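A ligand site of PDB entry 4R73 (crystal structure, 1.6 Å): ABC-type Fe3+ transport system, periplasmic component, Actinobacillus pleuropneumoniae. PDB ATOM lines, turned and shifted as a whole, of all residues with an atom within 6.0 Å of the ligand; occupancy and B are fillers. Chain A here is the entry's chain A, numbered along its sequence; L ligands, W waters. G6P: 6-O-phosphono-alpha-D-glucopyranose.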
ATOM      1  N   SER A  11      18.965  21.874 -15.060  1.00  0.00           N
ATOM      2  CA  SER A  11      19.760  22.935 -15.652  1.00  0.00           C
ATOM      3  C   SER A  11      19.130  23.506 -16.901  1.00  0.00           C
ATOM      4  O   SER A  11      19.768  24.251 -17.624  1.00  0.00           O
ATOM      5  CB  SER A  11      21.177  22.439 -15.968  1.00  0.00           C
ATOM      6  OG  SER A  11      21.898  22.064 -14.786  1.00  0.00           O
ATOM      7  N   ALA A  12      17.888  23.108 -17.159  1.00  0.00           N
ATOM      8  CA  ALA A  12      17.082  23.742 -18.214  1.00  0.00           C
ATOM      9  C   ALA A  12      16.423  24.992 -17.642  1.00  0.00           C
ATOM     10  O   ALA A  12      16.745  25.429 -16.533  1.00  0.00           O
ATOM     11  CB  ALA A  12      16.034  22.751 -18.742  1.00  0.00           C
ATOM     12  N   THR A  13      15.541  25.603 -18.406  1.00  0.00           N
ATOM     13  CA  THR A  13      14.804  26.736 -17.856  1.00  0.00           C
ATOM     14  C   THR A  13      13.828  26.329 -16.764  1.00  0.00           C
ATOM     15  O   THR A  13      13.312  25.204 -16.776  1.00  0.00           O
ATOM     16  CB  THR A  13      14.001  27.460 -18.917  1.00  0.00           C
ATOM     17  OG1 THR A  13      13.161  26.517 -19.602  1.00  0.00           O
ATOM     18  CG2 THR A  13      14.902  28.142 -19.920  1.00  0.00           C
ATOM     19  N   ARG A  36      17.091  24.564  -9.613  1.00  0.00           N
ATOM     20  CA  ARG A  36      17.659  24.879 -10.929  1.00  0.00           C
ATOM     21  C   ARG A  36      18.910  25.710 -10.791  1.00  0.00           C
ATOM     22  O   ARG A  36      19.032  26.617  -9.960  1.00  0.00           O
ATOM     23  CB  ARG A  36      16.673  25.606 -11.864  1.00  0.00           C
ATOM     24  CG  ARG A  36      17.120  25.612 -13.373  1.00  0.00           C
ATOM     25  CD  ARG A  36      17.999  26.814 -13.855  1.00  0.00           C
ATOM     26  NE  ARG A  36      18.750  26.525 -15.083  1.00  0.00           N
ATOM     27  CZ  ARG A  36      19.840  27.191 -15.487  1.00  0.00           C
ATOM     28  NH1 ARG A  36      20.296  28.213 -14.767  1.00  0.00           N
ATOM     29  NH2 ARG A  36      20.489  26.839 -16.616  1.00  0.00           N
ATOM     30  N   ASN A  37      19.891  25.322 -11.600  1.00  0.00           N
ATOM     31  CA  ASN A  37      21.165  26.024 -11.659  1.00  0.00           C
ATOM     32  C   ASN A  37      21.843  25.755 -12.988  1.00  0.00           C
ATOM     33  O   ASN A  37      21.481  24.787 -13.694  1.00  0.00           O
ATOM     34  CB  ASN A  37      22.053  25.589 -10.505  1.00  0.00           C
ATOM     35  CG  ASN A  37      22.922  26.722  -9.994  1.00  0.00           C
ATOM     36  OD1 ASN A  37      23.230  27.673 -10.711  1.00  0.00           O
ATOM     37  ND2 ASN A  37      23.309  26.640  -8.730  1.00  0.00           N
ATOM     38  N   GLY A  38      22.846  26.570 -13.322  1.00  0.00           N
ATOM     39  CA  GLY A  38      23.533  26.442 -14.600  1.00  0.00           C
ATOM     40  C   GLY A  38      24.219  25.095 -14.740  1.00  0.00           C
ATOM     41  O   GLY A  38      24.481  24.406 -13.734  1.00  0.00           O
ATOM     42  N   SER A  39      24.537  24.715 -15.979  1.00  0.00           N
ATOM     43  CA  SER A  39      25.174  23.397 -16.210  1.00  0.00           C
ATOM     44  C   SER A  39      26.523  23.285 -15.494  1.00  0.00           C
ATOM     45  O   SER A  39      26.837  22.251 -14.896  1.00  0.00           O
ATOM     46  CB  SER A  39      25.360  23.139 -17.704  1.00  0.00           C
ATOM     47  OG  SER A  39      24.172  23.423 -18.419  1.00  0.00           O
ATOM     48  N   GLY A  40      27.338  24.333 -15.612  1.00  0.00           N
ATOM     49  CA  GLY A  40      28.640  24.343 -14.952  1.00  0.00           C
ATOM     50  C   GLY A  40      28.502  24.475 -13.445  1.00  0.00           C
ATOM     51  O   GLY A  40      29.229  23.791 -12.686  1.00  0.00           O
ATOM     52  N   GLY A  60      18.670  18.166 -17.931  1.00  0.00           N
ATOM     53  CA  GLY A  60      18.803  19.342 -18.757  1.00  0.00           C
ATOM     54  C   GLY A  60      20.130  20.015 -18.565  1.00  0.00           C
ATOM     55  O   GLY A  60      21.009  19.549 -17.850  1.00  0.00           O
ATOM     56  N   GLY A  61      20.274  21.125 -19.251  1.00  0.00           N
ATOM     57  CA  GLY A  61      21.571  21.726 -19.359  1.00  0.00           C
ATOM     58  C   GLY A  61      22.383  20.953 -20.370  1.00  0.00           C
ATOM     59  O   GLY A  61      21.953  19.947 -20.899  1.00  0.00           O
ATOM     60  N   THR A  62      23.576  21.432 -20.637  1.00  0.00           N
ATOM     61  CA  THR A  62      24.382  20.825 -21.686  1.00  0.00           C
ATOM     62  C   THR A  62      25.050  19.514 -21.236  1.00  0.00           C
ATOM     63  O   THR A  62      25.315  19.267 -20.043  1.00  0.00           O
ATOM     64  CB  THR A  62      25.460  21.784 -22.191  1.00  0.00           C
ATOM     65  OG1 THR A  62      26.409  22.011 -21.129  1.00  0.00           O
ATOM     66  CG2 THR A  62      24.838  23.139 -22.570  1.00  0.00           C
ATOM     67  N   TYR A 105      17.622  16.226 -25.657  1.00  0.00           N
ATOM     68  CA  TYR A 105      17.224  17.222 -26.659  1.00  0.00           C
ATOM     69  C   TYR A 105      18.480  17.741 -27.327  1.00  0.00           C
ATOM     70  O   TYR A 105      19.600  17.408 -26.936  1.00  0.00           O
ATOM     71  CB  TYR A 105      16.398  18.369 -26.034  1.00  0.00           C
ATOM     72  CG  TYR A 105      17.008  19.171 -24.894  1.00  0.00           C
ATOM     73  CD1 TYR A 105      18.077  20.041 -25.096  1.00  0.00           C
ATOM     74  CD2 TYR A 105      16.462  19.090 -23.626  1.00  0.00           C
ATOM     75  CE1 TYR A 105      18.592  20.834 -24.033  1.00  0.00           C
ATOM     76  CE2 TYR A 105      16.956  19.839 -22.572  1.00  0.00           C
ATOM     77  CZ  TYR A 105      18.038  20.691 -22.770  1.00  0.00           C
ATOM     78  OH  TYR A 105      18.465  21.421 -21.688  1.00  0.00           O
ATOM     79  N   GLY A 107      20.110  21.469 -28.920  1.00  0.00           N
ATOM     80  CA  GLY A 107      19.980  22.920 -29.002  1.00  0.00           C
ATOM     81  C   GLY A 107      21.060  23.441 -29.946  1.00  0.00           C
ATOM     82  O   GLY A 107      22.228  23.097 -29.783  1.00  0.00           O
ATOM     83  N   ALA A 145      27.131  34.190 -22.162  1.00  0.00           N
ATOM     84  CA  ALA A 145      27.286  33.797 -20.770  1.00  0.00           C
ATOM     85  C   ALA A 145      28.770  33.466 -20.439  1.00  0.00           C
ATOM     86  O   ALA A 145      29.638  33.401 -21.320  1.00  0.00           O
ATOM     87  CB  ALA A 145      26.378  32.609 -20.457  1.00  0.00           C
ATOM     88  N   SER A 149      29.901  29.210 -15.129  1.00  0.00           N
ATOM     89  CA  SER A 149      28.582  28.795 -14.671  1.00  0.00           C
ATOM     90  C   SER A 149      27.789  28.124 -15.766  1.00  0.00           C
ATOM     91  O   SER A 149      27.053  27.158 -15.511  1.00  0.00           O
ATOM     92  CB  SER A 149      27.798  30.008 -14.135  1.00  0.00           C
ATOM     93  OG  SER A 149      27.915  31.115 -15.022  1.00  0.00           O
ATOM     94  N   SER A 150      27.953  28.636 -16.976  1.00  0.00           N
ATOM     95  CA  SER A 150      27.075  28.278 -18.101  1.00  0.00           C
ATOM     96  C   SER A 150      27.605  27.208 -19.053  1.00  0.00           C
ATOM     97  O   SER A 150      28.729  27.306 -19.603  1.00  0.00           O
ATOM     98  CB  SER A 150      26.775  29.555 -18.888  1.00  0.00           C
ATOM     99  OG  SER A 150      26.212  29.242 -20.175  1.00  0.00           O
ATOM    100  N   GLY A 151      26.775  26.194 -19.291  1.00  0.00           N
ATOM    101  CA  GLY A 151      27.064  25.184 -20.274  1.00  0.00           C
ATOM    102  C   GLY A 151      27.080  25.759 -21.684  1.00  0.00           C
ATOM    103  O   GLY A 151      27.898  25.396 -22.529  1.00  0.00           O
ATOM    104  N   THR A 152      26.138  26.668 -21.949  1.00  0.00           N
ATOM    105  CA  THR A 152      26.054  27.323 -23.254  1.00  0.00           C
ATOM    106  C   THR A 152      27.370  27.982 -23.640  1.00  0.00           C
ATOM    107  O   THR A 152      27.840  27.847 -24.773  1.00  0.00           O
ATOM    108  CB  THR A 152      24.906  28.390 -23.226  1.00  0.00           C
ATOM    109  OG1 THR A 152      23.683  27.823 -22.728  1.00  0.00           O
ATOM    110  CG2 THR A 152      24.682  28.993 -24.615  1.00  0.00           C
ATOM    111  N   ALA A 153      27.957  28.695 -22.671  1.00  0.00           N
ATOM    112  CA  ALA A 153      29.191  29.412 -22.936  1.00  0.00           C
ATOM    113  C   ALA A 153      30.299  28.402 -23.275  1.00  0.00           C
ATOM    114  O   ALA A 153      31.126  28.645 -24.149  1.00  0.00           O
ATOM    115  CB  ALA A 153      29.589  30.284 -21.721  1.00  0.00           C
ATOM    116  N   LYS A 185      25.468  35.110 -16.051  1.00  0.00           N
ATOM    117  CA  LYS A 185      25.641  33.877 -15.309  1.00  0.00           C
ATOM    118  C   LYS A 185      24.947  32.745 -16.055  1.00  0.00           C
ATOM    119  O   LYS A 185      25.524  31.675 -16.213  1.00  0.00           O
ATOM    120  CB  LYS A 185      25.074  33.958 -13.904  1.00  0.00           C
ATOM    121  CG  LYS A 185      25.192  32.657 -13.141  1.00  0.00           C
ATOM    122  CD  LYS A 185      24.906  32.887 -11.673  1.00  0.00           C
ATOM    123  CE  LYS A 185      25.132  31.609 -10.881  1.00  0.00           C
ATOM    124  NZ  LYS A 185      23.995  30.666 -11.110  1.00  0.00           N
ATOM    125  N   SER A 186      23.725  33.025 -16.505  1.00  0.00           N
ATOM    126  CA  SER A 186      22.902  32.019 -17.197  1.00  0.00           C
ATOM    127  C   SER A 186      23.029  32.093 -18.701  1.00  0.00           C
ATOM    128  O   SER A 186      23.101  33.180 -19.276  1.00  0.00           O
ATOM    129  CB  SER A 186      21.416  32.191 -16.833  1.00  0.00           C
ATOM    130  OG  SER A 186      21.209  32.039 -15.424  1.00  0.00           O
ATOM    131  N   GLY A 187      23.023  30.926 -19.339  1.00  0.00           N
ATOM    132  CA  GLY A 187      23.099  30.845 -20.792  1.00  0.00           C
ATOM    133  C   GLY A 187      22.030  31.645 -21.511  1.00  0.00           C
ATOM    134  O   GLY A 187      22.277  32.212 -22.572  1.00  0.00           O
ATOM    135  N   ILE A 188      20.828  31.635 -20.944  1.00  0.00           N
ATOM    136  CA  ILE A 188      19.643  32.199 -21.616  1.00  0.00           C
ATOM    137  C   ILE A 188      19.542  33.724 -21.462  1.00  0.00           C
ATOM    138  O   ILE A 188      18.767  34.383 -22.154  1.00  0.00           O
ATOM    139  CB  ILE A 188      18.386  31.541 -21.091  1.00  0.00           C
ATOM    140  CG1 ILE A 188      17.161  31.896 -21.966  1.00  0.00           C
ATOM    141  CG2 ILE A 188      18.124  31.978 -19.650  1.00  0.00           C
ATOM    142  CD1 ILE A 188      15.960  31.075 -21.650  1.00  0.00           C
ATOM    143  N   PHE A 205      21.601  29.476 -27.428  1.00  0.00           N
ATOM    144  CA  PHE A 205      20.949  28.416 -28.188  1.00  0.00           C
ATOM    145  C   PHE A 205      19.690  28.952 -28.824  1.00  0.00           C
ATOM    146  O   PHE A 205      18.883  29.601 -28.156  1.00  0.00           O
ATOM    147  CB  PHE A 205      20.641  27.218 -27.298  1.00  0.00           C
ATOM    148  CG  PHE A 205      21.876  26.521 -26.803  1.00  0.00           C
ATOM    149  CD1 PHE A 205      22.778  25.987 -27.710  1.00  0.00           C
ATOM    150  CD2 PHE A 205      22.080  26.335 -25.439  1.00  0.00           C
ATOM    151  CE1 PHE A 205      23.933  25.321 -27.243  1.00  0.00           C
ATOM    152  CE2 PHE A 205      23.235  25.669 -24.973  1.00  0.00           C
ATOM    153  CZ  PHE A 205      24.133  25.179 -25.868  1.00  0.00           C
ATOM    154  N   HIS A 207      16.872  27.972 -29.892  1.00  0.00           N
ATOM    155  CA  HIS A 207      15.478  27.736 -29.487  1.00  0.00           C
ATOM    156  C   HIS A 207      15.007  28.723 -28.421  1.00  0.00           C
ATOM    157  O   HIS A 207      13.821  28.973 -28.297  1.00  0.00           O
ATOM    158  CB  HIS A 207      15.274  26.292 -29.004  1.00  0.00           C
ATOM    159  CG  HIS A 207      16.140  25.933 -27.844  1.00  0.00           C
ATOM    160  ND1 HIS A 207      17.370  25.314 -28.008  1.00  0.00           N
ATOM    161  CD2 HIS A 207      16.008  26.164 -26.512  1.00  0.00           C
ATOM    162  CE1 HIS A 207      17.936  25.134 -26.833  1.00  0.00           C
ATOM    163  NE2 HIS A 207      17.146  25.646 -25.908  1.00  0.00           N
ATOM    164  N   ASP A 208      15.926  29.284 -27.625  1.00  0.00           N
ATOM    165  CA  ASP A 208      15.509  30.277 -26.603  1.00  0.00           C
ATOM    166  C   ASP A 208      15.131  31.559 -27.290  1.00  0.00           C
ATOM    167  O   ASP A 208      14.174  32.228 -26.878  1.00  0.00           O
ATOM    168  CB  ASP A 208      16.670  30.553 -25.602  1.00  0.00           C
ATOM    169  CG  ASP A 208      16.955  29.362 -24.711  1.00  0.00           C
ATOM    170  OD1 ASP A 208      16.036  28.592 -24.345  1.00  0.00           O
ATOM    171  OD2 ASP A 208      18.147  29.206 -24.363  1.00  0.00           O
ATOM    172  N   GLU A 231      24.354  21.834 -28.381  1.00  0.00           N
ATOM    173  CA  GLU A 231      24.306  21.023 -27.172  1.00  0.00           C
ATOM    174  C   GLU A 231      23.479  19.785 -27.416  1.00  0.00           C
ATOM    175  O   GLU A 231      22.537  19.798 -28.233  1.00  0.00           O
ATOM    176  CB  GLU A 231      23.669  21.800 -26.013  1.00  0.00           C
ATOM    177  CG  GLU A 231      22.246  22.334 -26.379  1.00  0.00           C
ATOM    178  CD  GLU A 231      21.452  22.797 -25.139  1.00  0.00           C
ATOM    179  OE1 GLU A 231      21.842  22.574 -23.964  1.00  0.00           O
ATOM    180  OE2 GLU A 231      20.383  23.416 -25.342  1.00  0.00           O
ATOM    181  N   GLY A 233      21.109  18.084 -24.648  1.00  0.00           N
ATOM    182  CA  GLY A 233      20.637  18.207 -23.282  1.00  0.00           C
ATOM    183  C   GLY A 233      20.872  16.870 -22.606  1.00  0.00           C
ATOM    184  O   GLY A 233      20.584  15.846 -23.202  1.00  0.00           O
ATOM    185  N   ALA A 269       9.551  25.109 -24.053  1.00  0.00           N
ATOM    186  CA  ALA A 269      10.929  24.796 -24.355  1.00  0.00           C
ATOM    187  C   ALA A 269      10.973  24.158 -25.744  1.00  0.00           C
ATOM    188  O   ALA A 269      10.412  23.083 -25.961  1.00  0.00           O
ATOM    189  CB  ALA A 269      11.520  23.863 -23.271  1.00  0.00           C
ATOM    190  N   GLN A 271      13.464  23.047 -27.800  1.00  0.00           N
ATOM    191  CA  GLN A 271      14.591  22.267 -28.325  1.00  0.00           C
ATOM    192  C   GLN A 271      14.106  21.180 -29.271  1.00  0.00           C
ATOM    193  O   GLN A 271      12.924  20.752 -29.232  1.00  0.00           O
ATOM    194  CB  GLN A 271      15.372  21.612 -27.163  1.00  0.00           C
ATOM    195  CG  GLN A 271      15.928  22.536 -26.124  1.00  0.00           C
ATOM    196  CD  GLN A 271      15.026  22.686 -24.912  1.00  0.00           C
ATOM    197  OE1 GLN A 271      13.828  22.422 -24.990  1.00  0.00           O
ATOM    198  NE2 GLN A 271      15.582  23.147 -23.792  1.00  0.00           N
HETATM  199  C1  G6P L   1      18.619  27.036 -21.620  1.00  0.00           C
HETATM  200  C2  G6P L   1      18.244  26.223 -22.740  1.00  0.00           C
HETATM  201  C3  G6P L   1      18.667  24.790 -22.520  1.00  0.00           C
HETATM  202  C4  G6P L   1      20.129  24.695 -22.146  1.00  0.00           C
HETATM  203  C5  G6P L   1      20.343  25.574 -20.934  1.00  0.00           C
HETATM  204  C6  G6P L   1      21.786  25.711 -20.559  1.00  0.00           C
HETATM  205  O1  G6P L   1      18.205  28.324 -21.639  1.00  0.00           O
HETATM  206  O2  G6P L   1      16.814  26.294 -23.007  1.00  0.00           O
HETATM  207  O3  G6P L   1      18.405  24.157 -23.731  1.00  0.00           O
HETATM  208  O4  G6P L   1      20.421  23.363 -21.906  1.00  0.00           O
HETATM  209  O5  G6P L   1      19.895  26.835 -21.243  1.00  0.00           O
HETATM  210  O6  G6P L   1      21.886  26.580 -19.483  1.00  0.00           O
HETATM  211  P   G6P L   1      23.310  27.195 -18.939  1.00  0.00           P
HETATM  212  O1P G6P L   1      22.894  28.238 -17.947  1.00  0.00           O
HETATM  213  O2P G6P L   1      24.081  26.105 -18.381  1.00  0.00           O
HETATM  214  O3P G6P L   1      23.995  27.743 -20.067  1.00  0.00           O
HETATM  215  O   HOH W   1      14.858  24.895 -21.366  1.00  0.00           O
HETATM  216  O   HOH W   2      24.532  29.109 -15.978  1.00  0.00           O
HETATM  217  O   HOH W   3      18.086  28.379 -18.268  1.00  0.00           O
HETATM  218  O   HOH W   4      21.288  29.079 -22.802  1.00  0.00           O
HETATM  219  O   HOH W   5      20.290  29.225 -19.275  1.00  0.00           O
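The side-chain carboxylate of Glu 231 is in hydrogen-bond range of an oxygen (O4) of the ligand (2.6 Å).
The side-chain hydroxyl of Ser 150 sits at hydrogen-bond distance from an oxygen (O3P) of the ligand, at 2.7 Å.
N of Thr 152 sits at hydrogen-bond distance from O3P of the ligand.
The side-chain hydroxyl (OG1) of Thr 152 is in hydrogen-bond range of an oxygen (O3P) of the ligand.
N of Ser 39 lies within hydrogen-bond range of O2P of the ligand, at 2.8 Å.
The side-chain hydroxyl (OG) of Ser 39 sits at hydrogen-bond distance from an oxygen (O2P) of the ligand (2.7 Å).
The side-chain hydroxyl (OH) of Tyr 105 lies within hydrogen-bond range of an oxygen (O4) of the ligand, 2.8 Å away.
The side-chain carboxylate of Asp 208 is in hydrogen-bond range of an oxygen (O2) of the ligand.
The backbone NH (N) of Gly 151 lies within hydrogen-bond range of an oxygen (O2P) of the ligand (2.8 Å).
An oxygen (O3) of the ligand sits at hydrogen-bond distance from a ring nitrogen (NE2) of His 207, at 2.9 Å.
O3 of the ligand lies within hydrogen-bond range of NE2 of Gln 271, 3.0 Å away.
An oxygen (O1P) of the ligand lies within hydrogen-bond range of the backbone NH of Gly 187 (3.0 Å).
The guanidinium group of Arg 36 lies within salt-bridge range of an oxygen (O1P) of the ligand (3.1 Å).
O4 of the ligand sits close to N of Gly 61 (3.5 Å).
The side-chain hydroxyl of Ser 150 is in hydrogen-bond range of the backbone NH of Thr 152 (3.1 Å).
The side-chain hydroxyl (OG) of Ser 150 is in hydrogen-bond range of the backbone NH (N) of Ala 153.
OG of Ser 39 is in hydrogen-bond range of N of Thr 62.
The side-chain hydroxyl (OH) of Tyr 105 sits at hydrogen-bond distance from the backbone NH (N) of Gly 61, at 3.0 Å.
The backbone NH of Gly 233 lies within hydrogen-bond range of the backbone carbonyl oxygen of Tyr 105.
The guanidinium group of Arg 36 lies within hydrogen-bond range of the backbone carbonyl oxygen of Ser 11.
The guanidinium group (NE) of Arg 36 sits at hydrogen-bond distance from the backbone carbonyl oxygen (O) of Ala 12 (2.7 Å).
OG of Ser 11 sits at hydrogen-bond distance from O of Asn 37.
Residues that only touch the ligand: Ser 11, Thr 13, Gly 38, Thr 62, Ser 186 and Ile 188.
Of the 30 residues printed, 18 come within 4 Å of the ligand.
Water W2 lies within hydrogen-bond range of O1P of the ligand, O of Lys 185 and O of Ser 149.
Water W1 lies within hydrogen-bond range of O2 of the ligand (2.9 Å), OG1 of Thr 13 (2.9 Å) and NE2 of Gln 271 (3.1 Å).
Water W4 lies within hydrogen-bond range of OG1 of Thr 152 (2.7 Å), O5 of the ligand (3.1 Å), N of Ile 188 (3.2 Å) and O of Gly 187 (3.3 Å).
Water W5 lies within hydrogen-bond range of the backbone NH of Ile 188, an oxygen (O1P) of the ligand and the backbone NH of Gly 187.
Water W3 bridges the guanidinium group of Arg 36 and an oxygen (O1) of the ligand.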
